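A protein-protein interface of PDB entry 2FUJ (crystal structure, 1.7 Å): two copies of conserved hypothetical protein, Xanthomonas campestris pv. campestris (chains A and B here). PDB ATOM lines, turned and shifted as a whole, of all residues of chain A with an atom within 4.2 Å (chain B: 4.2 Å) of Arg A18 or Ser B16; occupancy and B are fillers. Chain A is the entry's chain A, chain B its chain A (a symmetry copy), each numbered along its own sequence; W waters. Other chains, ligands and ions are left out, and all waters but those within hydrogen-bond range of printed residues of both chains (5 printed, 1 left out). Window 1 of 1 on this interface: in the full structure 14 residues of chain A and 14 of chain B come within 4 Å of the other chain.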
ATOM      1  N   SER A  16       3.757  17.398 -26.033  1.00  0.00           N
ATOM      2  CA  SER A  16       3.672  15.973 -26.287  1.00  0.00           C
ATOM      3  C   SER A  16       4.321  15.216 -25.140  1.00  0.00           C
ATOM      4  O   SER A  16       5.409  15.571 -24.703  1.00  0.00           O
ATOM      5  CB  SER A  16       4.420  15.608 -27.568  1.00  0.00           C
ATOM      6  OG  SER A  16       3.840  16.218 -28.693  1.00  0.00           O
ATOM      7  N   VAL A  17       3.654  14.175 -24.659  1.00  0.00           N
ATOM      8  CA  VAL A  17       4.212  13.355 -23.593  1.00  0.00           C
ATOM      9  C   VAL A  17       5.079  12.291 -24.264  1.00  0.00           C
ATOM     10  O   VAL A  17       4.777  11.853 -25.376  1.00  0.00           O
ATOM     11  CB  VAL A  17       3.100  12.662 -22.763  1.00  0.00           C
ATOM     12  CG1 VAL A  17       3.700  11.605 -21.843  1.00  0.00           C
ATOM     13  CG2 VAL A  17       2.371  13.692 -21.935  1.00  0.00           C
ATOM     14  N   ARG A  18       6.152  11.886 -23.594  1.00  0.00           N
ATOM     15  CA  ARG A  18       7.047  10.868 -24.124  1.00  0.00           C
ATOM     16  C   ARG A  18       6.915   9.608 -23.284  1.00  0.00           C
ATOM     17  O   ARG A  18       6.609   9.672 -22.099  1.00  0.00           O
ATOM     18  CB  ARG A  18       8.498  11.355 -24.095  1.00  0.00           C
ATOM     19  CG  ARG A  18       8.835  12.472 -25.060  1.00  0.00           C
ATOM     20  CD  ARG A  18      10.237  12.973 -24.786  1.00  0.00           C
ATOM     21  NE  ARG A  18      10.576  14.176 -25.543  1.00  0.00           N
ATOM     22  CZ  ARG A  18      11.693  14.873 -25.363  1.00  0.00           C
ATOM     23  NH1 ARG A  18      12.576  14.485 -24.453  1.00  0.00           N
ATOM     24  NH2 ARG A  18      11.929  15.955 -26.087  1.00  0.00           N
ATOM     25  N   TRP A  19       7.145   8.460 -23.909  1.00  0.00           N
ATOM     26  CA  TRP A  19       7.037   7.187 -23.222  1.00  0.00           C
ATOM     27  C   TRP A  19       7.971   7.162 -22.010  1.00  0.00           C
ATOM     28  O   TRP A  19       7.603   6.662 -20.945  1.00  0.00           O
ATOM     29  CB  TRP A  19       7.372   6.047 -24.190  1.00  0.00           C
ATOM     30  CG  TRP A  19       7.102   4.686 -23.648  1.00  0.00           C
ATOM     31  CD1 TRP A  19       5.899   4.047 -23.580  1.00  0.00           C
ATOM     32  CD2 TRP A  19       8.059   3.808 -23.057  1.00  0.00           C
ATOM     33  NE1 TRP A  19       6.049   2.817 -22.979  1.00  0.00           N
ATOM     34  CE2 TRP A  19       7.369   2.647 -22.651  1.00  0.00           C
ATOM     35  CE3 TRP A  19       9.437   3.888 -22.830  1.00  0.00           C
ATOM     36  CZ2 TRP A  19       8.013   1.575 -22.028  1.00  0.00           C
ATOM     37  CZ3 TRP A  19      10.072   2.824 -22.211  1.00  0.00           C
ATOM     38  CH2 TRP A  19       9.361   1.685 -21.818  1.00  0.00           C
ATOM     39  N   ARG A  20       9.177   7.695 -22.184  1.00  0.00           N
ATOM     40  CA  ARG A  20      10.175   7.750 -21.110  1.00  0.00           C
ATOM     41  C   ARG A  20       9.728   8.624 -19.928  1.00  0.00           C
ATOM     42  O   ARG A  20      10.339   8.584 -18.860  1.00  0.00           O
ATOM     43  CB  ARG A  20      11.505   8.272 -21.678  1.00  0.00           C
ATOM     44  CG  ARG A  20      12.556   8.676 -20.654  1.00  0.00           C
ATOM     45  CD  ARG A  20      13.006   7.496 -19.808  1.00  0.00           C
ATOM     46  NE  ARG A  20      13.821   7.919 -18.678  1.00  0.00           N
ATOM     47  CZ  ARG A  20      13.796   7.339 -17.482  1.00  0.00           C
ATOM     48  NH1 ARG A  20      13.002   6.302 -17.257  1.00  0.00           N
ATOM     49  NH2 ARG A  20      14.536   7.823 -16.495  1.00  0.00           N
ATOM     50  N   ASP A  21       8.671   9.413 -20.126  1.00  0.00           N
ATOM     51  CA  ASP A  21       8.166  10.291 -19.070  1.00  0.00           C
ATOM     52  C   ASP A  21       7.581   9.481 -17.923  1.00  0.00           C
ATOM     53  O   ASP A  21       7.519   9.951 -16.791  1.00  0.00           O
ATOM     54  CB  ASP A  21       7.082  11.231 -19.613  1.00  0.00           C
ATOM     55  CG  ASP A  21       7.642  12.373 -20.457  1.00  0.00           C
ATOM     56  OD1 ASP A  21       6.830  13.076 -21.086  1.00  0.00           O
ATOM     57  OD2 ASP A  21       8.868  12.583 -20.491  1.00  0.00           O
ATOM     58  N   MET A  22       7.135   8.267 -18.222  1.00  0.00           N
ATOM     59  CA  MET A  22       6.553   7.422 -17.191  1.00  0.00           C
ATOM     60  C   MET A  22       7.623   6.747 -16.341  1.00  0.00           C
ATOM     61  O   MET A  22       8.759   6.577 -16.775  1.00  0.00           O
ATOM     62  CB  MET A  22       5.650   6.349 -17.820  1.00  0.00           C
ATOM     63  CG  MET A  22       4.470   6.905 -18.632  1.00  0.00           C
ATOM     64  SD  MET A  22       3.285   5.612 -19.132  1.00  0.00           S
ATOM     65  CE  MET A  22       4.231   4.751 -20.388  1.00  0.00           C
ATOM     66  N   TRP A  74       1.072   7.794 -20.961  1.00  0.00           N
ATOM     67  CA  TRP A  74       1.387   7.908 -22.373  1.00  0.00           C
ATOM     68  C   TRP A  74       0.335   7.017 -23.040  1.00  0.00           C
ATOM     69  O   TRP A  74      -0.092   6.022 -22.453  1.00  0.00           O
ATOM     70  CB  TRP A  74       2.800   7.370 -22.600  1.00  0.00           C
ATOM     71  CG  TRP A  74       3.287   7.400 -24.007  1.00  0.00           C
ATOM     72  CD1 TRP A  74       4.038   8.371 -24.596  1.00  0.00           C
ATOM     73  CD2 TRP A  74       3.112   6.372 -24.986  1.00  0.00           C
ATOM     74  NE1 TRP A  74       4.353   8.007 -25.885  1.00  0.00           N
ATOM     75  CE2 TRP A  74       3.793   6.785 -26.150  1.00  0.00           C
ATOM     76  CE3 TRP A  74       2.449   5.139 -24.992  1.00  0.00           C
ATOM     77  CZ2 TRP A  74       3.828   6.009 -27.311  1.00  0.00           C
ATOM     78  CZ3 TRP A  74       2.485   4.366 -26.146  1.00  0.00           C
ATOM     79  CH2 TRP A  74       3.170   4.806 -27.288  1.00  0.00           C
ATOM     80  N   ILE B  15       9.344  14.728 -33.778  1.00  0.00           N
ATOM     81  CA  ILE B  15       9.488  14.754 -32.330  1.00  0.00           C
ATOM     82  C   ILE B  15       9.873  16.158 -31.904  1.00  0.00           C
ATOM     83  O   ILE B  15      10.781  16.753 -32.475  1.00  0.00           O
ATOM     84  CB  ILE B  15      10.604  13.785 -31.859  1.00  0.00           C
ATOM     85  CG1 ILE B  15      10.254  12.343 -32.238  1.00  0.00           C
ATOM     86  CG2 ILE B  15      10.812  13.906 -30.356  1.00  0.00           C
ATOM     87  CD1 ILE B  15      11.316  11.285 -31.914  1.00  0.00           C
ATOM     88  N   SER B  16       9.175  16.686 -30.906  1.00  0.00           N
ATOM     89  CA  SER B  16       9.476  18.010 -30.397  1.00  0.00           C
ATOM     90  C   SER B  16      10.632  17.922 -29.414  1.00  0.00           C
ATOM     91  O   SER B  16      10.645  17.052 -28.552  1.00  0.00           O
ATOM     92  CB  SER B  16       8.274  18.587 -29.651  1.00  0.00           C
ATOM     93  OG  SER B  16       7.175  18.764 -30.508  1.00  0.00           O
ATOM     94  N   VAL B  17      11.596  18.824 -29.545  1.00  0.00           N
ATOM     95  CA  VAL B  17      12.722  18.855 -28.623  1.00  0.00           C
ATOM     96  C   VAL B  17      12.295  19.714 -27.434  1.00  0.00           C
ATOM     97  O   VAL B  17      11.517  20.656 -27.595  1.00  0.00           O
ATOM     98  CB  VAL B  17      13.981  19.479 -29.279  1.00  0.00           C
ATOM     99  CG1 VAL B  17      15.051  19.755 -28.229  1.00  0.00           C
ATOM    100  CG2 VAL B  17      14.531  18.533 -30.319  1.00  0.00           C
ATOM    101  N   ARG B  18      12.794  19.383 -26.248  1.00  0.00           N
ATOM    102  CA  ARG B  18      12.470  20.133 -25.044  1.00  0.00           C
ATOM    103  C   ARG B  18      13.712  20.874 -24.575  1.00  0.00           C
ATOM    104  O   ARG B  18      14.831  20.428 -24.800  1.00  0.00           O
ATOM    105  CB  ARG B  18      11.982  19.196 -23.937  1.00  0.00           C
ATOM    106  CG  ARG B  18      10.630  18.553 -24.169  1.00  0.00           C
ATOM    107  CD  ARG B  18      10.370  17.518 -23.096  1.00  0.00           C
ATOM    108  NE  ARG B  18       9.175  16.715 -23.349  1.00  0.00           N
ATOM    109  CZ  ARG B  18       8.827  15.659 -22.622  1.00  0.00           C
ATOM    110  NH1 ARG B  18       9.581  15.280 -21.600  1.00  0.00           N
ATOM    111  NH2 ARG B  18       7.729  14.981 -22.915  1.00  0.00           N
ATOM    112  N   ASP B  21      16.224  19.070 -22.695  1.00  0.00           N
ATOM    113  CA  ASP B  21      16.982  18.074 -23.453  1.00  0.00           C
ATOM    114  C   ASP B  21      18.446  18.472 -23.563  1.00  0.00           C
ATOM    115  O   ASP B  21      19.315  17.625 -23.742  1.00  0.00           O
ATOM    116  CB  ASP B  21      16.408  17.910 -24.866  1.00  0.00           C
ATOM    117  CG  ASP B  21      15.105  17.116 -24.900  1.00  0.00           C
ATOM    118  OD1 ASP B  21      14.475  17.088 -25.972  1.00  0.00           O
ATOM    119  OD2 ASP B  21      14.712  16.516 -23.883  1.00  0.00           O
ATOM    120  N   LYS B  32      19.832  11.717 -24.794  1.00  0.00           N
ATOM    121  CA  LYS B  32      18.483  12.041 -25.231  1.00  0.00           C
ATOM    122  C   LYS B  32      18.209  11.517 -26.644  1.00  0.00           C
ATOM    123  O   LYS B  32      17.060  11.292 -27.019  1.00  0.00           O
ATOM    124  CB  LYS B  32      18.259  13.555 -25.171  1.00  0.00           C
ATOM    125  CG  LYS B  32      16.994  13.927 -24.432  1.00  0.00           C
ATOM    126  CD  LYS B  32      17.037  13.360 -23.020  1.00  0.00           C
ATOM    127  CE  LYS B  32      15.758  13.641 -22.261  1.00  0.00           C
ATOM    128  NZ  LYS B  32      14.582  13.043 -22.939  1.00  0.00           N
ATOM    129  N   TYR B  36      14.955   9.782 -28.273  1.00  0.00           N
ATOM    130  CA  TYR B  36      14.199  10.209 -29.451  1.00  0.00           C
ATOM    131  C   TYR B  36      13.920   8.977 -30.308  1.00  0.00           C
ATOM    132  O   TYR B  36      12.839   8.827 -30.875  1.00  0.00           O
ATOM    133  CB  TYR B  36      14.995  11.213 -30.290  1.00  0.00           C
ATOM    134  CG  TYR B  36      15.285  12.535 -29.625  1.00  0.00           C
ATOM    135  CD1 TYR B  36      14.385  13.098 -28.717  1.00  0.00           C
ATOM    136  CD2 TYR B  36      16.434  13.251 -29.939  1.00  0.00           C
ATOM    137  CE1 TYR B  36      14.628  14.343 -28.140  1.00  0.00           C
ATOM    138  CE2 TYR B  36      16.688  14.499 -29.372  1.00  0.00           C
ATOM    139  CZ  TYR B  36      15.779  15.040 -28.473  1.00  0.00           C
ATOM    140  OH  TYR B  36      16.023  16.274 -27.918  1.00  0.00           O
ATOM    141  N   GLU B  39      11.091   6.950 -28.639  1.00  0.00           N
ATOM    142  CA  GLU B  39       9.769   7.526 -28.879  1.00  0.00           C
ATOM    143  C   GLU B  39       9.286   7.202 -30.290  1.00  0.00           C
ATOM    144  O   GLU B  39       8.136   6.824 -30.489  1.00  0.00           O
ATOM    145  CB  GLU B  39       9.802   9.044 -28.682  1.00  0.00           C
ATOM    146  CG  GLU B  39       8.418   9.707 -28.618  1.00  0.00           C
ATOM    147  CD  GLU B  39       7.557   9.187 -27.475  1.00  0.00           C
ATOM    148  OE1 GLU B  39       8.120   8.690 -26.476  1.00  0.00           O
ATOM    149  OE2 GLU B  39       6.311   9.288 -27.569  1.00  0.00           O
ATOM    150  N   ASP B  77      12.919  21.393 -33.577  1.00  0.00           N
ATOM    151  CA  ASP B  77      12.287  20.081 -33.489  1.00  0.00           C
ATOM    152  C   ASP B  77      12.844  19.190 -34.595  1.00  0.00           C
ATOM    153  O   ASP B  77      13.313  19.686 -35.617  1.00  0.00           O
ATOM    154  CB  ASP B  77      10.768  20.213 -33.603  1.00  0.00           C
ATOM    155  CG  ASP B  77      10.183  21.085 -32.510  1.00  0.00           C
ATOM    156  OD1 ASP B  77      10.630  20.951 -31.347  1.00  0.00           O
ATOM    157  OD2 ASP B  77       9.278  21.896 -32.807  1.00  0.00           O
HETATM  158  O   HOH W   1       8.750  15.329 -27.315  1.00  0.00           O
HETATM  159  O   HOH W   2       7.589  17.160 -25.604  1.00  0.00           O
HETATM  160  O   HOH W   3       6.557  15.473 -30.347  1.00  0.00           O
HETATM  161  O   HOH W   4       5.311  19.109 -27.848  1.00  0.00           O
HETATM  162  O   HOH W   5      10.325   8.079 -24.871  1.00  0.00           O
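Water W2 bridges NE of Arg B18 (2.8 Å) and O of Ser A16 (2.8 Å). Water W1 lies within hydrogen-bond range of NE of Arg A18 (2.8 Å) and O of Ser B16 (2.8 Å). Water W5 lies within hydrogen-bond range of the side-chain carboxylate of Glu B39 (2.8 Å), the backbone NH of Arg A20 (2.9 Å) and the backbone NH of Trp A19 (3.3 Å). Water W4 lies within hydrogen-bond range of the backbone NH (N) of Ser A16 (2.9 Å) and the side-chain hydroxyl (OG) of Ser B16 (3.3 Å). Water W3 bridges N of Ser B16 and OG of Ser A16.
Of the printed residues of chain B, Trp A19 touches Glu B39 (2.8 Å). Of the printed residues of chain A, Ser B16 touches Arg A18. Printed residues of chain A within 4 Å of Val B17: Arg A18 (3.9 Å). Of the printed residues of chain A, Arg B18 touches Ser A16, Val A17, Arg A18 and Asp A21. Printed residues of chain A within 4 Å of Tyr B36: Arg A18. The nearest printed residue of chain A that does not touch Ser B16 is Ser A16 (4.6 Å). The nearest printed residue of chain B that does not touch Ser A16 is Ser B16 (4.6 Å).
OD1 of Asp A21 lies within hydrogen-bond range of N of Arg A18 (2.9 Å). SD of Met A22 sits at hydrogen-bond distance from N of Trp A74 (3.6 Å). The backbone NH (N) of Val B17 is in hydrogen-bond range of the side-chain carboxylate (OD1) of Asp B77, at 3.0 Å. OD1 of Asp B21 lies within hydrogen-bond range of N of Arg B18. The side-chain carboxylate of Asp B21 lies within salt-bridge range of the side-chain amino group of Lys B32, 3.6 Å away. The side-chain carboxylate (OD1) of Asp B21 lies within hydrogen-bond range of the side-chain hydroxyl (OH) of Tyr B36 (2.6 Å).
Ser A16 touches Arg B18, and with the chains exchanged Arg A18 touches Ser B16. Val A17 touches Arg B18, and with the chains exchanged Arg A18 touches Val B17. Arg B18 touches its own counterpart, Arg A18. Arg A18 touches Asp B21, and with the chains exchanged Asp A21 touches Arg B18. Of the 13 pairs that touch across the chains among the printed residues, 7 have their exchanged pair printed and touching as well.
Val A17 touches Arg B18. OE2 of Glu B39 touches O of Val A17, 3.7 Å away. NH2 of Arg A18 touches CA of Val B17, at 3.9 Å. Arg B18 touches Arg A18 (CG to NH2, 3.5 Å). Tyr B36 touches Arg A18. Glu B39 touches Arg A18 (OE1 to CA, 3.4 Å).
Of the 9 printed residues of chain B, 7 touch a printed residue of chain A. Printed residues of chain B that touch a printed residue of chain A: Ser B16, Val B17, Arg B18, Asp B21, Lys B32, Tyr B36 and Glu B39. Hydrophobic or aromatic side chains of chain B that line the printed part of chain A: Tyr B36. Of the 8 printed residues of chain A, 6 touch a printed residue of chain B. Among the printed residues, 13 pairs touch across the chains. Among the printed residues, Asp or Glu carboxylates within 4 Å of a Lys or Arg side-chain nitrogen of the other chain: Arg A18 with Asp B21 and Asp A21 with Arg B18.
NH2 of Arg B18 lies within hydrogen-bond range of O of Ser A16 (3.0 Å). NH2 of Arg A18 sits at hydrogen-bond distance from O of Ser B16 (3.0 Å). The guanidinium group (NH2) of Arg A18 is in salt-bridge range of the side-chain carboxylate (OD1) of Asp B21, at 2.8 Å. The side-chain carboxylate (OE1) of Glu B39 lies within hydrogen-bond range of the backbone NH (N) of Trp A19 (2.8 Å). The side-chain carboxylate (OD1) of Asp A21 lies within salt-bridge range of the guanidinium group (NH2) of Arg B18 (2.8 Å). The side-chain carboxylate (OE2) of Glu B39 lies within hydrogen-bond range of the indole nitrogen (NE1) of Trp A74, at 2.9 Å. NZ of Lys B32 lies close to NH1 of Arg A18 (2.9 Å).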
